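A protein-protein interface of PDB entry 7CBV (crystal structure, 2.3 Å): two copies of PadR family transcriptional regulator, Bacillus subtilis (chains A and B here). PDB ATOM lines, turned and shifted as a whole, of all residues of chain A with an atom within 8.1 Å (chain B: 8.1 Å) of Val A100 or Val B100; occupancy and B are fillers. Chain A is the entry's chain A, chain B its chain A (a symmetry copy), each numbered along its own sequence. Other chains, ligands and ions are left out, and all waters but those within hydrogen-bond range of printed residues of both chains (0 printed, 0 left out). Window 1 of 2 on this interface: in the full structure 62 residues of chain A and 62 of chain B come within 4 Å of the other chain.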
ATOM      1  N   GLN A  38      17.807   3.125   8.750  1.00  0.00           N
ATOM      2  CA  GLN A  38      18.981   2.990   9.592  1.00  0.00           C
ATOM      3  C   GLN A  38      18.571   2.503  10.971  1.00  0.00           C
ATOM      4  O   GLN A  38      19.065   1.475  11.432  1.00  0.00           O
ATOM      5  CB  GLN A  38      19.754   4.309   9.655  1.00  0.00           C
ATOM      6  CG  GLN A  38      20.377   4.722   8.317  1.00  0.00           C
ATOM      7  CD  GLN A  38      21.606   3.897   7.938  1.00  0.00           C
ATOM      8  OE1 GLN A  38      22.236   4.147   6.910  1.00  0.00           O
ATOM      9  NE2 GLN A  38      21.955   2.919   8.768  1.00  0.00           N
ATOM     10  N   PHE A  39      17.572   3.151  11.576  1.00  0.00           N
ATOM     11  CA  PHE A  39      17.066   2.840  12.911  1.00  0.00           C
ATOM     12  C   PHE A  39      15.731   2.089  12.888  1.00  0.00           C
ATOM     13  O   PHE A  39      15.160   1.803  13.956  1.00  0.00           O
ATOM     14  CB  PHE A  39      16.913   4.133  13.708  1.00  0.00           C
ATOM     15  CG  PHE A  39      15.978   5.107  13.067  1.00  0.00           C
ATOM     16  CD1 PHE A  39      16.392   5.872  11.985  1.00  0.00           C
ATOM     17  CD2 PHE A  39      14.670   5.237  13.519  1.00  0.00           C
ATOM     18  CE1 PHE A  39      15.531   6.759  11.376  1.00  0.00           C
ATOM     19  CE2 PHE A  39      13.797   6.129  12.916  1.00  0.00           C
ATOM     20  CZ  PHE A  39      14.230   6.896  11.845  1.00  0.00           C
ATOM     21  N   TRP A  40      15.195   1.801  11.698  1.00  0.00           N
ATOM     22  CA  TRP A  40      13.959   1.023  11.583  1.00  0.00           C
ATOM     23  C   TRP A  40      13.978   0.356  10.205  1.00  0.00           C
ATOM     24  O   TRP A  40      13.454   0.867   9.216  1.00  0.00           O
ATOM     25  CB  TRP A  40      12.714   1.884  11.795  1.00  0.00           C
ATOM     26  CG  TRP A  40      11.500   1.100  12.202  1.00  0.00           C
ATOM     27  CD1 TRP A  40      10.538   0.593  11.377  1.00  0.00           C
ATOM     28  CD2 TRP A  40      11.131   0.709  13.533  1.00  0.00           C
ATOM     29  NE1 TRP A  40       9.591  -0.077  12.110  1.00  0.00           N
ATOM     30  CE2 TRP A  40       9.928  -0.022  13.435  1.00  0.00           C
ATOM     31  CE3 TRP A  40      11.693   0.918  14.797  1.00  0.00           C
ATOM     32  CZ2 TRP A  40       9.280  -0.553  14.552  1.00  0.00           C
ATOM     33  CZ3 TRP A  40      11.057   0.388  15.904  1.00  0.00           C
ATOM     34  CH2 TRP A  40       9.859  -0.343  15.775  1.00  0.00           C
ATOM     35  N   SER A  41      14.649  -0.784  10.127  1.00  0.00           N
ATOM     36  CA  SER A  41      14.748  -1.508   8.869  1.00  0.00           C
ATOM     37  C   SER A  41      13.442  -2.236   8.554  1.00  0.00           C
ATOM     38  O   SER A  41      12.726  -2.704   9.446  1.00  0.00           O
ATOM     39  CB  SER A  41      15.889  -2.513   8.913  1.00  0.00           C
ATOM     40  OG  SER A  41      15.544  -3.537   9.818  1.00  0.00           O
ATOM     41  N   PRO A  97      12.218  -0.614  26.176  1.00  0.00           N
ATOM     42  CA  PRO A  97      12.432  -2.036  25.871  1.00  0.00           C
ATOM     43  C   PRO A  97      13.571  -2.641  26.676  1.00  0.00           C
ATOM     44  O   PRO A  97      14.400  -1.942  27.261  1.00  0.00           O
ATOM     45  CB  PRO A  97      12.772  -2.033  24.375  1.00  0.00           C
ATOM     46  CG  PRO A  97      12.305  -0.680  23.863  1.00  0.00           C
ATOM     47  CD  PRO A  97      12.476   0.254  25.011  1.00  0.00           C
ATOM     48  N   GLU A  98      13.571  -3.975  26.730  1.00  0.00           N
ATOM     49  CA  GLU A  98      14.755  -4.722  27.151  1.00  0.00           C
ATOM     50  C   GLU A  98      15.931  -4.407  26.226  1.00  0.00           C
ATOM     51  O   GLU A  98      15.754  -4.154  25.028  1.00  0.00           O
ATOM     52  CB  GLU A  98      14.467  -6.224  27.135  1.00  0.00           C
ATOM     53  N   THR A  99      17.139  -4.407  26.793  1.00  0.00           N
ATOM     54  CA  THR A  99      18.331  -4.013  26.036  1.00  0.00           C
ATOM     55  C   THR A  99      18.333  -4.648  24.654  1.00  0.00           C
ATOM     56  O   THR A  99      17.947  -5.805  24.478  1.00  0.00           O
ATOM     57  CB  THR A  99      19.625  -4.373  26.793  1.00  0.00           C
ATOM     58  OG1 THR A  99      19.763  -3.543  27.957  1.00  0.00           O
ATOM     59  CG2 THR A  99      20.871  -4.242  25.912  1.00  0.00           C
ATOM     60  N   VAL A 100      18.719  -3.849  23.664  1.00  0.00           N
ATOM     61  CA  VAL A 100      18.843  -4.341  22.304  1.00  0.00           C
ATOM     62  C   VAL A 100      20.012  -5.305  22.219  1.00  0.00           C
ATOM     63  O   VAL A 100      21.089  -5.058  22.785  1.00  0.00           O
ATOM     64  CB  VAL A 100      19.040  -3.165  21.336  1.00  0.00           C
ATOM     65  N   LYS A 101      19.799  -6.418  21.519  1.00  0.00           N
ATOM     66  CA  LYS A 101      20.850  -7.405  21.354  1.00  0.00           C
ATOM     67  C   LYS A 101      22.100  -6.750  20.788  1.00  0.00           C
ATOM     68  O   LYS A 101      22.027  -5.909  19.892  1.00  0.00           O
ATOM     69  CB  LYS A 101      20.379  -8.525  20.425  1.00  0.00           C
ATOM     70  CG  LYS A 101      19.848  -8.021  19.085  1.00  0.00           C
ATOM     71  CD  LYS A 101      19.664  -9.155  18.087  1.00  0.00           C
ATOM     72  CE  LYS A 101      20.811  -9.218  17.088  1.00  0.00           C
ATOM     73  NZ  LYS A 101      20.711 -10.437  16.237  1.00  0.00           N
ATOM     74  N   ASP A 102      23.247  -7.097  21.363  1.00  0.00           N
ATOM     75  CA  ASP A 102      24.532  -6.691  20.812  1.00  0.00           C
ATOM     76  C   ASP A 102      25.434  -7.909  20.916  1.00  0.00           C
ATOM     77  O   ASP A 102      25.838  -8.308  22.011  1.00  0.00           O
ATOM     78  CB  ASP A 102      25.117  -5.474  21.534  1.00  0.00           C
ATOM     79  CG  ASP A 102      26.399  -4.954  20.884  1.00  0.00           C
ATOM     80  OD1 ASP A 102      27.161  -5.737  20.266  1.00  0.00           O
ATOM     81  OD2 ASP A 102      26.655  -3.738  20.997  1.00  0.00           O
ATOM     82  N   GLU A 103      25.730  -8.504  19.771  1.00  0.00           N
ATOM     83  CA  GLU A 103      26.497  -9.732  19.761  1.00  0.00           C
ATOM     84  C   GLU A 103      27.904  -9.497  20.291  1.00  0.00           C
ATOM     85  O   GLU A 103      28.450 -10.329  21.026  1.00  0.00           O
ATOM     86  CB  GLU A 103      26.526 -10.289  18.347  1.00  0.00           C
ATOM     87  CG  GLU A 103      26.843 -11.754  18.285  1.00  0.00           C
ATOM     88  CD  GLU A 103      26.913 -12.264  16.865  1.00  0.00           C
ATOM     89  OE1 GLU A 103      26.498 -11.539  15.952  1.00  0.00           O
ATOM     90  OE2 GLU A 103      27.430 -13.375  16.657  1.00  0.00           O
ATOM     91  N   MET A 105      28.814  -7.544  22.591  1.00  0.00           N
ATOM     92  CA  MET A 105      28.800  -7.465  24.045  1.00  0.00           C
ATOM     93  C   MET A 105      28.615  -8.835  24.684  1.00  0.00           C
ATOM     94  O   MET A 105      29.041  -9.049  25.832  1.00  0.00           O
ATOM     95  CB  MET A 105      27.699  -6.515  24.491  1.00  0.00           C
ATOM     96  CG  MET A 105      28.035  -5.062  24.191  1.00  0.00           C
ATOM     97  SD  MET A 105      29.638  -4.470  24.823  1.00  0.00           S
ATOM     98  CE  MET A 105      29.522  -4.941  26.554  1.00  0.00           C
ATOM     99  N   LYS A 133      32.019   4.074  11.262  1.00  0.00           N
ATOM    100  CA  LYS A 133      30.594   4.363  11.227  1.00  0.00           C
ATOM    101  C   LYS A 133      30.313   5.765  11.762  1.00  0.00           C
ATOM    102  O   LYS A 133      29.542   6.517  11.160  1.00  0.00           O
ATOM    103  CB  LYS A 133      29.801   3.317  12.016  1.00  0.00           C
ATOM    104  CG  LYS A 133      28.314   3.544  11.929  1.00  0.00           C
ATOM    105  CD  LYS A 133      27.490   2.617  12.809  1.00  0.00           C
ATOM    106  CE  LYS A 133      25.986   2.846  12.537  1.00  0.00           C
ATOM    107  NZ  LYS A 133      25.082   2.150  13.509  1.00  0.00           N
ATOM    108  N   ARG A 170      25.299   8.204  20.033  1.00  0.00           N
ATOM    109  CA  ARG A 170      25.394   6.801  20.402  1.00  0.00           C
ATOM    110  C   ARG A 170      26.732   6.212  19.976  1.00  0.00           C
ATOM    111  O   ARG A 170      27.375   5.497  20.748  1.00  0.00           O
ATOM    112  CB  ARG A 170      24.224   6.018  19.798  1.00  0.00           C
ATOM    113  CG  ARG A 170      24.190   4.573  20.258  1.00  0.00           C
ATOM    114  CD  ARG A 170      23.015   3.789  19.680  1.00  0.00           C
ATOM    115  NE  ARG A 170      23.017   3.756  18.217  1.00  0.00           N
ATOM    116  CZ  ARG A 170      22.026   4.198  17.445  1.00  0.00           C
ATOM    117  NH1 ARG A 170      20.924   4.711  17.981  1.00  0.00           N
ATOM    118  NH2 ARG A 170      22.141   4.120  16.128  1.00  0.00           N
ATOM    119  N   GLU A 171      27.166   6.495  18.744  1.00  0.00           N
ATOM    120  CA  GLU A 171      28.449   5.978  18.274  1.00  0.00           C
ATOM    121  C   GLU A 171      29.626   6.616  19.000  1.00  0.00           C
ATOM    122  O   GLU A 171      30.604   5.927  19.287  1.00  0.00           O
ATOM    123  CB  GLU A 171      28.586   6.176  16.767  1.00  0.00           C
ATOM    124  CG  GLU A 171      27.624   5.336  15.993  1.00  0.00           C
ATOM    125  CD  GLU A 171      27.750   3.854  16.296  1.00  0.00           C
ATOM    126  OE1 GLU A 171      28.889   3.344  16.305  1.00  0.00           O
ATOM    127  OE2 GLU A 171      26.711   3.209  16.534  1.00  0.00           O
ATOM    128  N   GLN B  38      19.744  -9.262  30.236  1.00  0.00           N
ATOM    129  CA  GLN B  38      19.543  -7.837  30.050  1.00  0.00           C
ATOM    130  C   GLN B  38      19.875  -7.454  28.617  1.00  0.00           C
ATOM    131  O   GLN B  38      19.033  -6.886  27.922  1.00  0.00           O
ATOM    132  CB  GLN B  38      20.367  -7.039  31.062  1.00  0.00           C
ATOM    133  CG  GLN B  38      19.910  -7.231  32.514  1.00  0.00           C
ATOM    134  CD  GLN B  38      18.606  -6.505  32.842  1.00  0.00           C
ATOM    135  OE1 GLN B  38      18.142  -6.535  33.982  1.00  0.00           O
ATOM    136  NE2 GLN B  38      18.014  -5.848  31.849  1.00  0.00           N
ATOM    137  N   PHE B  39      21.042  -7.880  28.126  1.00  0.00           N
ATOM    138  CA  PHE B  39      21.536  -7.584  26.783  1.00  0.00           C
ATOM    139  C   PHE B  39      21.412  -8.770  25.820  1.00  0.00           C
ATOM    140  O   PHE B  39      21.840  -8.673  24.657  1.00  0.00           O
ATOM    141  CB  PHE B  39      22.995  -7.143  26.867  1.00  0.00           C
ATOM    142  CG  PHE B  39      23.885  -8.180  27.477  1.00  0.00           C
ATOM    143  CD1 PHE B  39      23.904  -8.367  28.852  1.00  0.00           C
ATOM    144  CD2 PHE B  39      24.676  -8.994  26.677  1.00  0.00           C
ATOM    145  CE1 PHE B  39      24.707  -9.334  29.422  1.00  0.00           C
ATOM    146  CE2 PHE B  39      25.489  -9.967  27.239  1.00  0.00           C
ATOM    147  CZ  PHE B  39      25.509 -10.132  28.616  1.00  0.00           C
ATOM    148  N   TRP B  40      20.878  -9.901  26.288  1.00  0.00           N
ATOM    149  CA  TRP B  40      20.654 -11.058  25.420  1.00  0.00           C
ATOM    150  C   TRP B  40      19.518 -11.874  26.044  1.00  0.00           C
ATOM    151  O   TRP B  40      19.723 -12.810  26.818  1.00  0.00           O
ATOM    152  CB  TRP B  40      21.924 -11.888  25.223  1.00  0.00           C
ATOM    153  CG  TRP B  40      21.907 -12.736  23.986  1.00  0.00           C
ATOM    154  CD1 TRP B  40      21.506 -14.038  23.892  1.00  0.00           C
ATOM    155  CD2 TRP B  40      22.282 -12.337  22.660  1.00  0.00           C
ATOM    156  NE1 TRP B  40      21.619 -14.476  22.596  1.00  0.00           N
ATOM    157  CE2 TRP B  40      22.093 -13.454  21.819  1.00  0.00           C
ATOM    158  CE3 TRP B  40      22.773 -11.150  22.105  1.00  0.00           C
ATOM    159  CZ2 TRP B  40      22.368 -13.418  20.451  1.00  0.00           C
ATOM    160  CZ3 TRP B  40      23.041 -11.109  20.749  1.00  0.00           C
ATOM    161  CH2 TRP B  40      22.835 -12.239  19.934  1.00  0.00           C
ATOM    162  N   SER B  41      18.292 -11.472  25.747  1.00  0.00           N
ATOM    163  CA  SER B  41      17.128 -12.159  26.287  1.00  0.00           C
ATOM    164  C   SER B  41      16.889 -13.480  25.559  1.00  0.00           C
ATOM    165  O   SER B  41      17.147 -13.621  24.358  1.00  0.00           O
ATOM    166  CB  SER B  41      15.887 -11.289  26.175  1.00  0.00           C
ATOM    167  OG  SER B  41      15.551 -11.167  24.811  1.00  0.00           O
ATOM    168  N   PRO B  97      26.085  -4.526  13.317  1.00  0.00           N
ATOM    169  CA  PRO B  97      24.703  -4.655  12.832  1.00  0.00           C
ATOM    170  C   PRO B  97      24.111  -3.324  12.396  1.00  0.00           C
ATOM    171  O   PRO B  97      24.620  -2.248  12.715  1.00  0.00           O
ATOM    172  CB  PRO B  97      23.949  -5.207  14.049  1.00  0.00           C
ATOM    173  CG  PRO B  97      25.027  -5.749  14.974  1.00  0.00           C
ATOM    174  CD  PRO B  97      26.215  -4.880  14.742  1.00  0.00           C
ATOM    175  N   GLU B  98      23.033  -3.420  11.615  1.00  0.00           N
ATOM    176  CA  GLU B  98      22.146  -2.280  11.394  1.00  0.00           C
ATOM    177  C   GLU B  98      21.573  -1.794  12.726  1.00  0.00           C
ATOM    178  O   GLU B  98      21.344  -2.583  13.652  1.00  0.00           O
ATOM    179  CB  GLU B  98      21.008  -2.670  10.449  1.00  0.00           C
ATOM    180  N   THR B  99      21.354  -0.482  12.827  1.00  0.00           N
ATOM    181  CA  THR B  99      20.911   0.118  14.088  1.00  0.00           C
ATOM    182  C   THR B  99      19.807  -0.712  14.728  1.00  0.00           C
ATOM    183  O   THR B  99      18.924  -1.237  14.047  1.00  0.00           O
ATOM    184  CB  THR B  99      20.443   1.573  13.890  1.00  0.00           C
ATOM    185  OG1 THR B  99      21.564   2.413  13.574  1.00  0.00           O
ATOM    186  CG2 THR B  99      19.709   2.123  15.117  1.00  0.00           C
ATOM    187  N   VAL B 100      19.905  -0.867  16.045  1.00  0.00           N
ATOM    188  CA  VAL B 100      18.881  -1.569  16.796  1.00  0.00           C
ATOM    189  C   VAL B 100      17.607  -0.742  16.811  1.00  0.00           C
ATOM    190  O   VAL B 100      17.641   0.484  16.995  1.00  0.00           O
ATOM    191  CB  VAL B 100      19.371  -1.834  18.229  1.00  0.00           C
ATOM    192  N   LYS B 101      16.476  -1.414  16.603  1.00  0.00           N
ATOM    193  CA  LYS B 101      15.195  -0.732  16.615  1.00  0.00           C
ATOM    194  C   LYS B 101      15.026   0.047  17.909  1.00  0.00           C
ATOM    195  O   LYS B 101      15.372  -0.434  18.989  1.00  0.00           O
ATOM    196  CB  LYS B 101      14.058  -1.745  16.459  1.00  0.00           C
ATOM    197  CG  LYS B 101      14.113  -2.881  17.478  1.00  0.00           C
ATOM    198  CD  LYS B 101      12.828  -3.696  17.484  1.00  0.00           C
ATOM    199  CE  LYS B 101      11.923  -3.311  18.646  1.00  0.00           C
ATOM    200  NZ  LYS B 101      10.598  -3.983  18.535  1.00  0.00           N
ATOM    201  N   ASP B 102      14.547   1.280  17.785  1.00  0.00           N
ATOM    202  CA  ASP B 102      14.164   2.072  18.946  1.00  0.00           C
ATOM    203  C   ASP B 102      12.861   2.758  18.571  1.00  0.00           C
ATOM    204  O   ASP B 102      12.839   3.665  17.733  1.00  0.00           O
ATOM    205  CB  ASP B 102      15.251   3.073  19.351  1.00  0.00           C
ATOM    206  CG  ASP B 102      14.923   3.818  20.645  1.00  0.00           C
ATOM    207  OD1 ASP B 102      13.729   4.028  20.971  1.00  0.00           O
ATOM    208  OD2 ASP B 102      15.877   4.207  21.347  1.00  0.00           O
ATOM    209  N   GLU B 103      11.780   2.308  19.185  1.00  0.00           N
ATOM    210  CA  GLU B 103      10.471   2.819  18.831  1.00  0.00           C
ATOM    211  C   GLU B 103      10.356   4.299  19.173  1.00  0.00           C
ATOM    212  O   GLU B 103       9.772   5.079  18.410  1.00  0.00           O
ATOM    213  CB  GLU B 103       9.408   2.005  19.545  1.00  0.00           C
ATOM    214  CG  GLU B 103       8.052   2.092  18.907  1.00  0.00           C
ATOM    215  CD  GLU B 103       7.009   1.312  19.672  1.00  0.00           C
ATOM    216  OE1 GLU B 103       7.381   0.528  20.555  1.00  0.00           O
ATOM    217  OE2 GLU B 103       5.809   1.516  19.419  1.00  0.00           O
ATOM    218  N   MET B 105      12.589   6.515  18.991  1.00  0.00           N
ATOM    219  CA  MET B 105      13.270   7.321  17.987  1.00  0.00           C
ATOM    220  C   MET B 105      12.478   7.394  16.689  1.00  0.00           C
ATOM    221  O   MET B 105      12.621   8.364  15.926  1.00  0.00           O
ATOM    222  CB  MET B 105      14.655   6.751  17.735  1.00  0.00           C
ATOM    223  CG  MET B 105      15.603   6.999  18.900  1.00  0.00           C
ATOM    224  SD  MET B 105      15.750   8.731  19.449  1.00  0.00           S
ATOM    225  CE  MET B 105      16.132   9.553  17.898  1.00  0.00           C
ATOM    226  N   LYS B 133      16.211   3.955  34.927  1.00  0.00           N
ATOM    227  CA  LYS B 133      16.973   2.786  34.514  1.00  0.00           C
ATOM    228  C   LYS B 133      18.460   2.986  34.794  1.00  0.00           C
ATOM    229  O   LYS B 133      19.119   2.086  35.321  1.00  0.00           O
ATOM    230  CB  LYS B 133      16.741   2.472  33.034  1.00  0.00           C
ATOM    231  CG  LYS B 133      17.453   1.219  32.599  1.00  0.00           C
ATOM    232  CD  LYS B 133      17.371   0.941  31.106  1.00  0.00           C
ATOM    233  CE  LYS B 133      18.013  -0.430  30.797  1.00  0.00           C
ATOM    234  NZ  LYS B 133      18.189  -0.702  29.334  1.00  0.00           N
ATOM    235  N   ARG B 170      25.840   3.685  28.118  1.00  0.00           N
ATOM    236  CA  ARG B 170      24.800   3.835  27.113  1.00  0.00           C
ATOM    237  C   ARG B 170      23.630   4.646  27.652  1.00  0.00           C
ATOM    238  O   ARG B 170      23.122   5.541  26.970  1.00  0.00           O
ATOM    239  CB  ARG B 170      24.344   2.460  26.619  1.00  0.00           C
ATOM    240  CG  ARG B 170      23.357   2.550  25.471  1.00  0.00           C
ATOM    241  CD  ARG B 170      22.911   1.184  24.955  1.00  0.00           C
ATOM    242  NE  ARG B 170      22.271   0.368  25.986  1.00  0.00           N
ATOM    243  CZ  ARG B 170      22.685  -0.838  26.370  1.00  0.00           C
ATOM    244  NH1 ARG B 170      23.750  -1.400  25.809  1.00  0.00           N
ATOM    245  NH2 ARG B 170      22.025  -1.483  27.319  1.00  0.00           N
ATOM    246  N   GLU B 171      23.184   4.346  28.875  1.00  0.00           N
ATOM    247  CA  GLU B 171      22.074   5.093  29.462  1.00  0.00           C
ATOM    248  C   GLU B 171      22.460   6.530  29.792  1.00  0.00           C
ATOM    249  O   GLU B 171      21.642   7.432  29.612  1.00  0.00           O
ATOM    250  CB  GLU B 171      21.553   4.386  30.710  1.00  0.00           C
ATOM    251  CG  GLU B 171      20.900   3.082  30.395  1.00  0.00           C
ATOM    252  CD  GLU B 171      19.756   3.214  29.403  1.00  0.00           C
ATOM    253  OE1 GLU B 171      18.907   4.111  29.592  1.00  0.00           O
ATOM    254  OE2 GLU B 171      19.715   2.428  28.439  1.00  0.00           O
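N of Thr B99 lies close to O of Gln A38. The backbone NH (N) of Thr A99 sits close to the backbone carbonyl oxygen (O) of Gln B38, at 3.3 Å. OG1 of Thr A99 sits at hydrogen-bond distance from NH2 of Arg B170 (3.1 Å). The side-chain hydroxyl (OG1) of Thr B99 lies within hydrogen-bond range of the guanidinium group (NH2) of Arg A170.
The side-chain carboxylate (OD1) of Asp A102 sits at hydrogen-bond distance from the backbone NH (N) of Met A105 (3.4 Å). OE2 of Glu A171 lies within salt-bridge range of NZ of Lys A133 (3.6 Å). OD1 of Asp B102 lies within hydrogen-bond range of N of Met B105 (3.4 Å). The side-chain carboxylate (OE2) of Glu B171 lies within salt-bridge range of the side-chain amino group (NZ) of Lys B133, 3.6 Å away.
Phe A39 touches Thr B99. Phe A39 touches Lys B101 (O to CA, 3.7 Å). Phe A39 touches Asp B102. Asp B102 touches Trp A40. CG2 of Thr A99 touches CA of Phe B39, at 3.5 Å. Thr A99 touches Lys B133 (OG1 to NZ, 3.5 Å). CZ3 of Trp B40 touches CB of Lys A101 (3.7 Å). Asp A102 touches Trp B40 (C to CZ3, 3.999 Å). Met A105 touches Phe B39 (O to CE2, 3.9 Å). NZ of Lys A133 touches OG1 of Thr B99 (3.5 Å).
Of chain B, only Val B100 comes within 4 Å of Val A100. Val B100 touches one residue of chain A. Printed residues of chain A within 4 Å of Met B105: Phe A39 (3.9 Å). Of the printed residues of chain A, Lys B133 touches Thr A99 (3.5 Å). Of the printed residues of chain A, Arg B170 touches Thr A99. The nearest residue of chain A that does not touch Val B100 is Phe A39 (4.1 Å).
Printed residues of chain A that touch a printed residue of chain B: Gln A38, Phe A39, Trp A40, Thr A99, Val A100, Lys A101, Asp A102, Glu A103, Met A105, Lys A133 and Arg A170. Hydrophobic or aromatic side chains of chain A that line the printed part of chain B: Phe A39, Trp A40 and Val A100. Among the printed residues, 21 pairs touch across the chains. Among the printed residues, no Asp or Glu carboxylate lies within 4 Å of a Lys or Arg side-chain nitrogen of the other chain.
Gln A38 touches Thr B99, and with the chains exchanged Thr A99 touches Gln B38. Phe A39 touches Asp B102, and with the chains exchanged Asp A102 touches Phe B39. Trp A40 touches Asp B102, and with the chains exchanged Asp A102 touches Trp B40. Trp A40 touches Glu B103, and with the chains exchanged Glu A103 touches Trp B40. Positions printed for both chains: 38, 39, 40, 41, 97, 98, 99, 100, 101, 102, 103, 105, 133, 170 and 171. Of the 21 pairs that touch across the chains among the printed residues, 21 have their exchanged pair printed and touching as well.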
